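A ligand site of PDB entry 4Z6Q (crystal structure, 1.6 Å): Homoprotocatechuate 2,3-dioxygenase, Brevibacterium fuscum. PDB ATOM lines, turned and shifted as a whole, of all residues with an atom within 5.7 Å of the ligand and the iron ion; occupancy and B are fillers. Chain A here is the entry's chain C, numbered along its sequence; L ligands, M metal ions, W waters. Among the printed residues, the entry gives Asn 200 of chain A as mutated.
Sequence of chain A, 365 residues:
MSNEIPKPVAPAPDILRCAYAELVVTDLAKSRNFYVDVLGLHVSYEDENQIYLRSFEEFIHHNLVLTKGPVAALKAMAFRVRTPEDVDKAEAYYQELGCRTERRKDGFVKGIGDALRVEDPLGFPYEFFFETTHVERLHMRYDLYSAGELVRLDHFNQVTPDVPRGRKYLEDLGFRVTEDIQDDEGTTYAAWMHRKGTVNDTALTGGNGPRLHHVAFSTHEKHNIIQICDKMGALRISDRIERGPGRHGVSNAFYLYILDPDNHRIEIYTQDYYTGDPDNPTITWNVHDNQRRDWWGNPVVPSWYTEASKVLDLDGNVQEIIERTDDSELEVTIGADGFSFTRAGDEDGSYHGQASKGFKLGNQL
Water W2 lies within hydrogen-bond range of OD1 of Asn 200 (2.5 Å) and OH of Tyr 269 (2.8 Å).
The guanidinium group (NH2) of Arg 243 lies within salt-bridge range of an oxygen (O1) of the ligand, at 2.7 Å. An oxygen (O3) of the ligand lies close to the side-chain hydroxyl (OH) of Tyr 257 (2.6 Å). An oxygen (O2) of the ligand lies within salt-bridge range of the guanidinium group (NH1) of Arg 293, 2.8 Å away. O of Arg 293 lies close to O1 of the ligand (3.0 Å). An oxygen (O1) of the ligand lies within hydrogen-bond range of a ring nitrogen (ND1) of His 248 (2.6 Å).
Of the 21 residues printed, 3 come within 4 Å of the iron ion. Along chain A the residues within 4 Å of the iron ion span positions 155 to 267. The nearest printed residue that does not touch the iron ion is Tyr 257 (4.1 Å).
Trp 192 touches the ligand (NE1 to C5, 3.3 Å). O of Val 250 touches C6 of the ligand (3.3 Å). Ser 251 touches the ligand (OG to C5, 3.6 Å). CE2 of Tyr 269 touches O4 of the ligand, at 3.4 Å. CH2 of Trp 304 touches O2 of the ligand, 3.6 Å away. Hydrophobic or aromatic side chains within 4 Å of the ligand: His 155, Trp 192, His 214, His 248, Val 250, Tyr 257, Tyr 269 and Trp 304.
The iron ion is bound by OE1 of Glu 267, 2.0 Å away. O3 of the ligand binds the iron ion (2.1 Å). The iron ion is bound by an oxygen (O4) of the ligand. NE2 of His 155 is bound to the iron ion (2.2 Å). NE2 of His 214 binds the iron ion (2.2 Å). The iron ion has five donor atoms within binding distance. Slightly farther from the iron ion lies water W1 (2.6 Å).
The backbone NH of Tyr 257 sits at hydrogen-bond distance from the backbone carbonyl oxygen of Arg 243 (2.9 Å). O of Arg 292 sits at hydrogen-bond distance from N of Val 250 (2.9 Å). O of His 214 is in hydrogen-bond range of N of Asn 157, at 3.0 Å. The backbone carbonyl oxygen of His 155 is in hydrogen-bond range of the backbone NH of Ala 216 (2.8 Å). OE2 of Glu 267 sits at hydrogen-bond distance from OH of Tyr 257, at 3.2 Å. The side-chain amide oxygen (OD1) of Asn 200 sits at hydrogen-bond distance from a ring nitrogen (ND1) of His 155, at 3.3 Å. The side-chain carboxylate of Glu 267 sits at hydrogen-bond distance from a ring nitrogen (NE2) of His 248. The backbone NH of Gly 249 lies within hydrogen-bond range of the backbone carbonyl oxygen of Arg 293 (2.9 Å).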
ATOM      1  N   HIS A 155     -10.045   9.393 -13.208  1.00  0.00           N
ATOM      2  CA  HIS A 155      -9.930  10.425 -14.251  1.00  0.00           C
ATOM      3  C   HIS A 155     -10.015  11.821 -13.702  1.00  0.00           C
ATOM      4  O   HIS A 155     -10.375  11.998 -12.529  1.00  0.00           O
ATOM      5  CB  HIS A 155     -11.012  10.215 -15.327  1.00  0.00           C
ATOM      6  CG  HIS A 155     -12.428  10.328 -14.835  1.00  0.00           C
ATOM      7  ND1 HIS A 155     -13.207   9.247 -14.475  1.00  0.00           N
ATOM      8  CD2 HIS A 155     -13.224  11.418 -14.734  1.00  0.00           C
ATOM      9  CE1 HIS A 155     -14.421   9.656 -14.184  1.00  0.00           C
ATOM     10  NE2 HIS A 155     -14.465  10.966 -14.347  1.00  0.00           N
ATOM     11  N   ASN A 157     -11.797  15.763 -15.015  1.00  0.00           N
ATOM     12  CA  ASN A 157     -12.750  16.372 -15.904  1.00  0.00           C
ATOM     13  C   ASN A 157     -12.537  17.881 -15.828  1.00  0.00           C
ATOM     14  O   ASN A 157     -12.486  18.471 -14.745  1.00  0.00           O
ATOM     15  CB  ASN A 157     -14.191  15.963 -15.564  1.00  0.00           C
ATOM     16  CG  ASN A 157     -15.198  16.464 -16.560  1.00  0.00           C
ATOM     17  OD1 ASN A 157     -15.262  17.691 -16.813  1.00  0.00           O
ATOM     18  ND2 ASN A 157     -15.952  15.563 -17.159  1.00  0.00           N
ATOM     19  N   ILE A 181     -21.228  14.348 -26.351  1.00  0.00           N
ATOM     20  CA  ILE A 181     -22.585  14.871 -26.399  1.00  0.00           C
ATOM     21  C   ILE A 181     -22.617  16.027 -27.398  1.00  0.00           C
ATOM     22  O   ILE A 181     -21.813  16.964 -27.307  1.00  0.00           O
ATOM     23  CB  ILE A 181     -23.016  15.381 -25.010  1.00  0.00           C
ATOM     24  CG1 ILE A 181     -23.077  14.208 -24.003  1.00  0.00           C
ATOM     25  CG2 ILE A 181     -24.351  16.077 -25.090  1.00  0.00           C
ATOM     26  CD1 ILE A 181     -23.254  14.626 -22.567  1.00  0.00           C
ATOM     27  N   TRP A 192     -15.289  12.744 -23.763  1.00  0.00           N
ATOM     28  CA  TRP A 192     -14.539  11.910 -22.843  1.00  0.00           C
ATOM     29  C   TRP A 192     -13.426  11.211 -23.629  1.00  0.00           C
ATOM     30  O   TRP A 192     -13.642  10.816 -24.736  1.00  0.00           O
ATOM     31  CB  TRP A 192     -15.472  10.855 -22.247  1.00  0.00           C
ATOM     32  CG  TRP A 192     -16.421  11.407 -21.216  1.00  0.00           C
ATOM     33  CD1 TRP A 192     -16.321  11.218 -19.872  1.00  0.00           C
ATOM     34  CD2 TRP A 192     -17.628  12.167 -21.424  1.00  0.00           C
ATOM     35  NE1 TRP A 192     -17.356  11.849 -19.219  1.00  0.00           N
ATOM     36  CE2 TRP A 192     -18.183  12.440 -20.157  1.00  0.00           C
ATOM     37  CE3 TRP A 192     -18.309  12.626 -22.557  1.00  0.00           C
ATOM     38  CZ2 TRP A 192     -19.353  13.156 -19.989  1.00  0.00           C
ATOM     39  CZ3 TRP A 192     -19.477  13.368 -22.388  1.00  0.00           C
ATOM     40  CH2 TRP A 192     -20.004  13.606 -21.126  1.00  0.00           C
ATOM     41  N   ASN A 200     -12.421   7.156 -19.691  1.00  0.00           N
ATOM     42  CA  ASN A 200     -11.633   8.394 -19.732  1.00  0.00           C
ATOM     43  C   ASN A 200     -10.475   8.413 -18.782  1.00  0.00           C
ATOM     44  O   ASN A 200     -10.460   7.725 -17.765  1.00  0.00           O
ATOM     45  CB  ASN A 200     -12.506   9.667 -19.657  1.00  0.00           C
ATOM     46  CG  ASN A 200     -13.196   9.838 -18.349  1.00  0.00           C
ATOM     47  OD1 ASN A 200     -13.682   8.868 -17.706  1.00  0.00           O
ATOM     48  ND2 ASN A 200     -13.295  11.104 -17.936  1.00  0.00           N
ATOM     49  N   HIS A 214     -13.932  18.078 -11.862  1.00  0.00           N
ATOM     50  CA  HIS A 214     -13.766  17.103 -10.778  1.00  0.00           C
ATOM     51  C   HIS A 214     -12.574  16.221 -10.949  1.00  0.00           C
ATOM     52  O   HIS A 214     -11.962  16.145 -12.035  1.00  0.00           O
ATOM     53  CB  HIS A 214     -15.003  16.225 -10.601  1.00  0.00           C
ATOM     54  CG  HIS A 214     -15.429  15.447 -11.813  1.00  0.00           C
ATOM     55  ND1 HIS A 214     -16.371  15.891 -12.699  1.00  0.00           N
ATOM     56  CD2 HIS A 214     -15.141  14.172 -12.202  1.00  0.00           C
ATOM     57  CE1 HIS A 214     -16.594  14.985 -13.625  1.00  0.00           C
ATOM     58  NE2 HIS A 214     -15.874  13.926 -13.329  1.00  0.00           N
ATOM     59  N   ALA A 216     -11.972  12.073 -10.193  1.00  0.00           N
ATOM     60  CA  ALA A 216     -12.765  10.849  -9.952  1.00  0.00           C
ATOM     61  C   ALA A 216     -11.931   9.706  -9.449  1.00  0.00           C
ATOM     62  O   ALA A 216     -10.870   9.416 -10.007  1.00  0.00           O
ATOM     63  CB  ALA A 216     -13.454  10.411 -11.220  1.00  0.00           C
ATOM     64  N   ARG A 243     -24.788  15.590  -6.202  1.00  0.00           N
ATOM     65  CA  ARG A 243     -25.555  14.970  -7.283  1.00  0.00           C
ATOM     66  C   ARG A 243     -25.336  13.477  -7.244  1.00  0.00           C
ATOM     67  O   ARG A 243     -24.221  13.029  -7.101  1.00  0.00           O
ATOM     68  CB  ARG A 243     -25.066  15.502  -8.622  1.00  0.00           C
ATOM     69  CG  ARG A 243     -25.676  14.809  -9.840  1.00  0.00           C
ATOM     70  CD  ARG A 243     -25.351  15.482 -11.182  1.00  0.00           C
ATOM     71  NE  ARG A 243     -25.774  14.540 -12.210  1.00  0.00           N
ATOM     72  CZ  ARG A 243     -25.090  14.163 -13.286  1.00  0.00           C
ATOM     73  NH1 ARG A 243     -24.046  14.864 -13.734  1.00  0.00           N
ATOM     74  NH2 ARG A 243     -25.509  13.107 -13.981  1.00  0.00           N
ATOM     75  N   HIS A 248     -24.719   6.527 -14.860  1.00  0.00           N
ATOM     76  CA  HIS A 248     -24.432   7.386 -15.987  1.00  0.00           C
ATOM     77  C   HIS A 248     -24.959   6.749 -17.295  1.00  0.00           C
ATOM     78  O   HIS A 248     -24.907   5.523 -17.501  1.00  0.00           O
ATOM     79  CB  HIS A 248     -22.931   7.556 -16.180  1.00  0.00           C
ATOM     80  CG  HIS A 248     -22.229   8.520 -15.278  1.00  0.00           C
ATOM     81  ND1 HIS A 248     -22.620   9.829 -15.054  1.00  0.00           N
ATOM     82  CD2 HIS A 248     -21.058   8.357 -14.589  1.00  0.00           C
ATOM     83  CE1 HIS A 248     -21.723  10.424 -14.267  1.00  0.00           C
ATOM     84  NE2 HIS A 248     -20.778   9.554 -13.985  1.00  0.00           N
ATOM     85  N   GLY A 249     -25.424   7.597 -18.208  1.00  0.00           N
ATOM     86  CA  GLY A 249     -25.612   7.225 -19.596  1.00  0.00           C
ATOM     87  C   GLY A 249     -24.284   7.092 -20.313  1.00  0.00           C
ATOM     88  O   GLY A 249     -23.753   5.993 -20.458  1.00  0.00           O
ATOM     89  N   VAL A 250     -23.704   8.240 -20.646  1.00  0.00           N
ATOM     90  CA  VAL A 250     -22.267   8.289 -20.994  1.00  0.00           C
ATOM     91  C   VAL A 250     -21.435   7.533 -19.958  1.00  0.00           C
ATOM     92  O   VAL A 250     -21.506   7.814 -18.777  1.00  0.00           O
ATOM     93  CB  VAL A 250     -21.732   9.739 -21.030  1.00  0.00           C
ATOM     94  CG1 VAL A 250     -20.205   9.754 -21.207  1.00  0.00           C
ATOM     95  CG2 VAL A 250     -22.404  10.508 -22.143  1.00  0.00           C
ATOM     96  N   SER A 251     -20.651   6.553 -20.435  1.00  0.00           N
ATOM     97  CA  SER A 251     -19.735   5.727 -19.641  1.00  0.00           C
ATOM     98  C   SER A 251     -20.372   4.476 -19.045  1.00  0.00           C
ATOM     99  O   SER A 251     -19.658   3.528 -18.754  1.00  0.00           O
ATOM    100  CB  SER A 251     -18.992   6.461 -18.522  1.00  0.00           C
ATOM    101  OG  SER A 251     -19.763   6.596 -17.332  1.00  0.00           O
ATOM    102  N   TYR A 255     -22.247   6.248 -10.222  1.00  0.00           N
ATOM    103  CA  TYR A 255     -21.556   7.494  -9.875  1.00  0.00           C
ATOM    104  C   TYR A 255     -22.169   8.243  -8.667  1.00  0.00           C
ATOM    105  O   TYR A 255     -23.291   8.006  -8.268  1.00  0.00           O
ATOM    106  CB  TYR A 255     -21.512   8.434 -11.074  1.00  0.00           C
ATOM    107  CG  TYR A 255     -22.822   9.112 -11.361  1.00  0.00           C
ATOM    108  CD1 TYR A 255     -23.741   8.546 -12.192  1.00  0.00           C
ATOM    109  CD2 TYR A 255     -23.137  10.323 -10.761  1.00  0.00           C
ATOM    110  CE1 TYR A 255     -24.964   9.165 -12.432  1.00  0.00           C
ATOM    111  CE2 TYR A 255     -24.337  10.950 -10.973  1.00  0.00           C
ATOM    112  CZ  TYR A 255     -25.255  10.378 -11.832  1.00  0.00           C
ATOM    113  OH  TYR A 255     -26.454  10.992 -12.026  1.00  0.00           O
ATOM    114  N   TYR A 257     -21.369  12.461  -6.970  1.00  0.00           N
ATOM    115  CA  TYR A 257     -20.569  13.674  -6.822  1.00  0.00           C
ATOM    116  C   TYR A 257     -20.720  14.306  -5.444  1.00  0.00           C
ATOM    117  O   TYR A 257     -21.834  14.574  -4.984  1.00  0.00           O
ATOM    118  CB  TYR A 257     -20.943  14.720  -7.881  1.00  0.00           C
ATOM    119  CG  TYR A 257     -20.714  14.273  -9.307  1.00  0.00           C
ATOM    120  CD1 TYR A 257     -19.465  14.361  -9.920  1.00  0.00           C
ATOM    121  CD2 TYR A 257     -21.749  13.701 -10.025  1.00  0.00           C
ATOM    122  CE1 TYR A 257     -19.281  13.932 -11.236  1.00  0.00           C
ATOM    123  CE2 TYR A 257     -21.592  13.293 -11.318  1.00  0.00           C
ATOM    124  CZ  TYR A 257     -20.364  13.389 -11.912  1.00  0.00           C
ATOM    125  OH  TYR A 257     -20.287  12.962 -13.204  1.00  0.00           O
ATOM    126  N   GLU A 267     -15.697  12.954  -7.777  1.00  0.00           N
ATOM    127  CA  GLU A 267     -16.610  11.944  -8.276  1.00  0.00           C
ATOM    128  C   GLU A 267     -16.162  10.577  -7.756  1.00  0.00           C
ATOM    129  O   GLU A 267     -14.969  10.282  -7.690  1.00  0.00           O
ATOM    130  CB  GLU A 267     -16.663  11.915  -9.799  1.00  0.00           C
ATOM    131  CG  GLU A 267     -17.712  10.906 -10.325  1.00  0.00           C
ATOM    132  CD  GLU A 267     -17.773  10.786 -11.827  1.00  0.00           C
ATOM    133  OE1 GLU A 267     -16.834  11.247 -12.513  1.00  0.00           O
ATOM    134  OE2 GLU A 267     -18.761  10.238 -12.338  1.00  0.00           O
ATOM    135  N   TYR A 269     -16.972   6.499  -8.672  1.00  0.00           N
ATOM    136  CA  TYR A 269     -17.242   5.979 -10.006  1.00  0.00           C
ATOM    137  C   TYR A 269     -16.913   4.499 -10.031  1.00  0.00           C
ATOM    138  O   TYR A 269     -15.943   4.068  -9.395  1.00  0.00           O
ATOM    139  CB  TYR A 269     -16.321   6.734 -10.974  1.00  0.00           C
ATOM    140  CG  TYR A 269     -16.359   6.493 -12.467  1.00  0.00           C
ATOM    141  CD1 TYR A 269     -15.559   5.497 -13.092  1.00  0.00           C
ATOM    142  CD2 TYR A 269     -17.111   7.316 -13.283  1.00  0.00           C
ATOM    143  CE1 TYR A 269     -15.547   5.359 -14.470  1.00  0.00           C
ATOM    144  CE2 TYR A 269     -17.059   7.188 -14.662  1.00  0.00           C
ATOM    145  CZ  TYR A 269     -16.270   6.223 -15.251  1.00  0.00           C
ATOM    146  OH  TYR A 269     -16.220   6.074 -16.618  1.00  0.00           O
ATOM    147  N   ARG A 292     -28.891  10.738 -21.047  1.00  0.00           N
ATOM    148  CA  ARG A 292     -27.464  10.805 -21.415  1.00  0.00           C
ATOM    149  C   ARG A 292     -26.516  10.975 -20.240  1.00  0.00           C
ATOM    150  O   ARG A 292     -25.379  10.548 -20.282  1.00  0.00           O
ATOM    151  CB  ARG A 292     -27.212  11.944 -22.435  1.00  0.00           C
ATOM    152  CG  ARG A 292     -27.174  13.334 -21.806  1.00  0.00           C
ATOM    153  CD  ARG A 292     -27.375  14.495 -22.748  1.00  0.00           C
ATOM    154  NE  ARG A 292     -27.317  15.709 -21.945  1.00  0.00           N
ATOM    155  CZ  ARG A 292     -28.303  16.123 -21.151  1.00  0.00           C
ATOM    156  NH1 ARG A 292     -29.477  15.484 -21.087  1.00  0.00           N
ATOM    157  NH2 ARG A 292     -28.113  17.216 -20.424  1.00  0.00           N
ATOM    158  N   ARG A 293     -26.961  11.717 -19.213  1.00  0.00           N
ATOM    159  CA  ARG A 293     -26.124  11.988 -18.073  1.00  0.00           C
ATOM    160  C   ARG A 293     -26.507  11.045 -16.938  1.00  0.00           C
ATOM    161  O   ARG A 293     -25.771  10.054 -16.708  1.00  0.00           O
ATOM    162  CB  ARG A 293     -26.155  13.465 -17.701  1.00  0.00           C
ATOM    163  CG  ARG A 293     -25.356  14.305 -18.694  1.00  0.00           C
ATOM    164  CD  ARG A 293     -24.960  15.695 -18.189  1.00  0.00           C
ATOM    165  NE  ARG A 293     -24.102  16.425 -19.139  1.00  0.00           N
ATOM    166  CZ  ARG A 293     -22.779  16.393 -19.167  1.00  0.00           C
ATOM    167  NH1 ARG A 293     -22.092  15.617 -18.357  1.00  0.00           N
ATOM    168  NH2 ARG A 293     -22.127  17.124 -20.066  1.00  0.00           N
ATOM    169  N   ASP A 294     -27.682  11.241 -16.361  1.00  0.00           N
ATOM    170  CA  ASP A 294     -28.248  10.229 -15.471  1.00  0.00           C
ATOM    171  C   ASP A 294     -29.186   9.337 -16.312  1.00  0.00           C
ATOM    172  O   ASP A 294     -30.196   9.786 -16.860  1.00  0.00           O
ATOM    173  CB  ASP A 294     -29.009  10.872 -14.352  1.00  0.00           C
ATOM    174  CG  ASP A 294     -29.405   9.861 -13.296  1.00  0.00           C
ATOM    175  OD1 ASP A 294     -28.527   9.498 -12.447  1.00  0.00           O
ATOM    176  OD2 ASP A 294     -30.556   9.399 -13.324  1.00  0.00           O
ATOM    177  N   VAL A 300     -30.202  16.939 -13.555  1.00  0.00           N
ATOM    178  CA  VAL A 300     -28.826  17.394 -13.239  1.00  0.00           C
ATOM    179  C   VAL A 300     -28.939  18.763 -12.546  1.00  0.00           C
ATOM    180  O   VAL A 300     -29.452  19.713 -13.121  1.00  0.00           O
ATOM    181  CB  VAL A 300     -27.960  17.504 -14.512  1.00  0.00           C
ATOM    182  CG1 VAL A 300     -26.562  17.981 -14.187  1.00  0.00           C
ATOM    183  CG2 VAL A 300     -27.912  16.136 -15.223  1.00  0.00           C
ATOM    184  N   TRP A 304     -23.936  21.695 -10.937  1.00  0.00           N
ATOM    185  CA  TRP A 304     -23.042  20.781 -11.694  1.00  0.00           C
ATOM    186  C   TRP A 304     -22.538  21.410 -13.011  1.00  0.00           C
ATOM    187  O   TRP A 304     -21.397  21.203 -13.427  1.00  0.00           O
ATOM    188  CB  TRP A 304     -23.747  19.450 -11.970  1.00  0.00           C
ATOM    189  CG  TRP A 304     -22.823  18.328 -12.247  1.00  0.00           C
ATOM    190  CD1 TRP A 304     -22.262  17.510 -11.323  1.00  0.00           C
ATOM    191  CD2 TRP A 304     -22.251  17.963 -13.505  1.00  0.00           C
ATOM    192  NE1 TRP A 304     -21.437  16.604 -11.925  1.00  0.00           N
ATOM    193  CE2 TRP A 304     -21.400  16.869 -13.275  1.00  0.00           C
ATOM    194  CE3 TRP A 304     -22.370  18.443 -14.804  1.00  0.00           C
ATOM    195  CZ2 TRP A 304     -20.676  16.256 -14.286  1.00  0.00           C
ATOM    196  CZ3 TRP A 304     -21.660  17.849 -15.798  1.00  0.00           C
ATOM    197  CH2 TRP A 304     -20.794  16.772 -15.528  1.00  0.00           C
HETATM  198  C1  LIG L   1     -20.783  11.796 -17.070  1.00  0.00           C
HETATM  199  C2  LIG L   1     -20.058  12.632 -16.187  1.00  0.00           C
HETATM  200  C3  LIG L   1     -18.857  12.165 -15.657  1.00  0.00           C
HETATM  201  C4  LIG L   1     -18.348  10.900 -16.083  1.00  0.00           C
HETATM  202  C5  LIG L   1     -19.050  10.124 -16.972  1.00  0.00           C
HETATM  203  C6  LIG L   1     -20.287  10.538 -17.462  1.00  0.00           C
HETATM  204  C7  LIG L   1     -22.170  12.189 -17.567  1.00  0.00           C
HETATM  205  C8  LIG L   1     -23.047  12.789 -16.465  1.00  0.00           C
HETATM  206  O1  LIG L   1     -23.763  12.043 -15.775  1.00  0.00           O
HETATM  207  O2  LIG L   1     -22.944  13.992 -16.283  1.00  0.00           O
HETATM  208  O3  LIG L   1     -18.190  12.889 -14.800  1.00  0.00           O
HETATM  209  O4  LIG L   1     -17.171  10.517 -15.545  1.00  0.00           O
HETATM  210 FE    FE M   1     -16.422  11.984 -14.282  1.00  0.00          FE
HETATM  211  O   HOH W   1     -15.551  12.755 -16.637  1.00  0.00           O
HETATM  212  O   HOH W   2     -16.099   8.796 -17.208  1.00  0.00           O
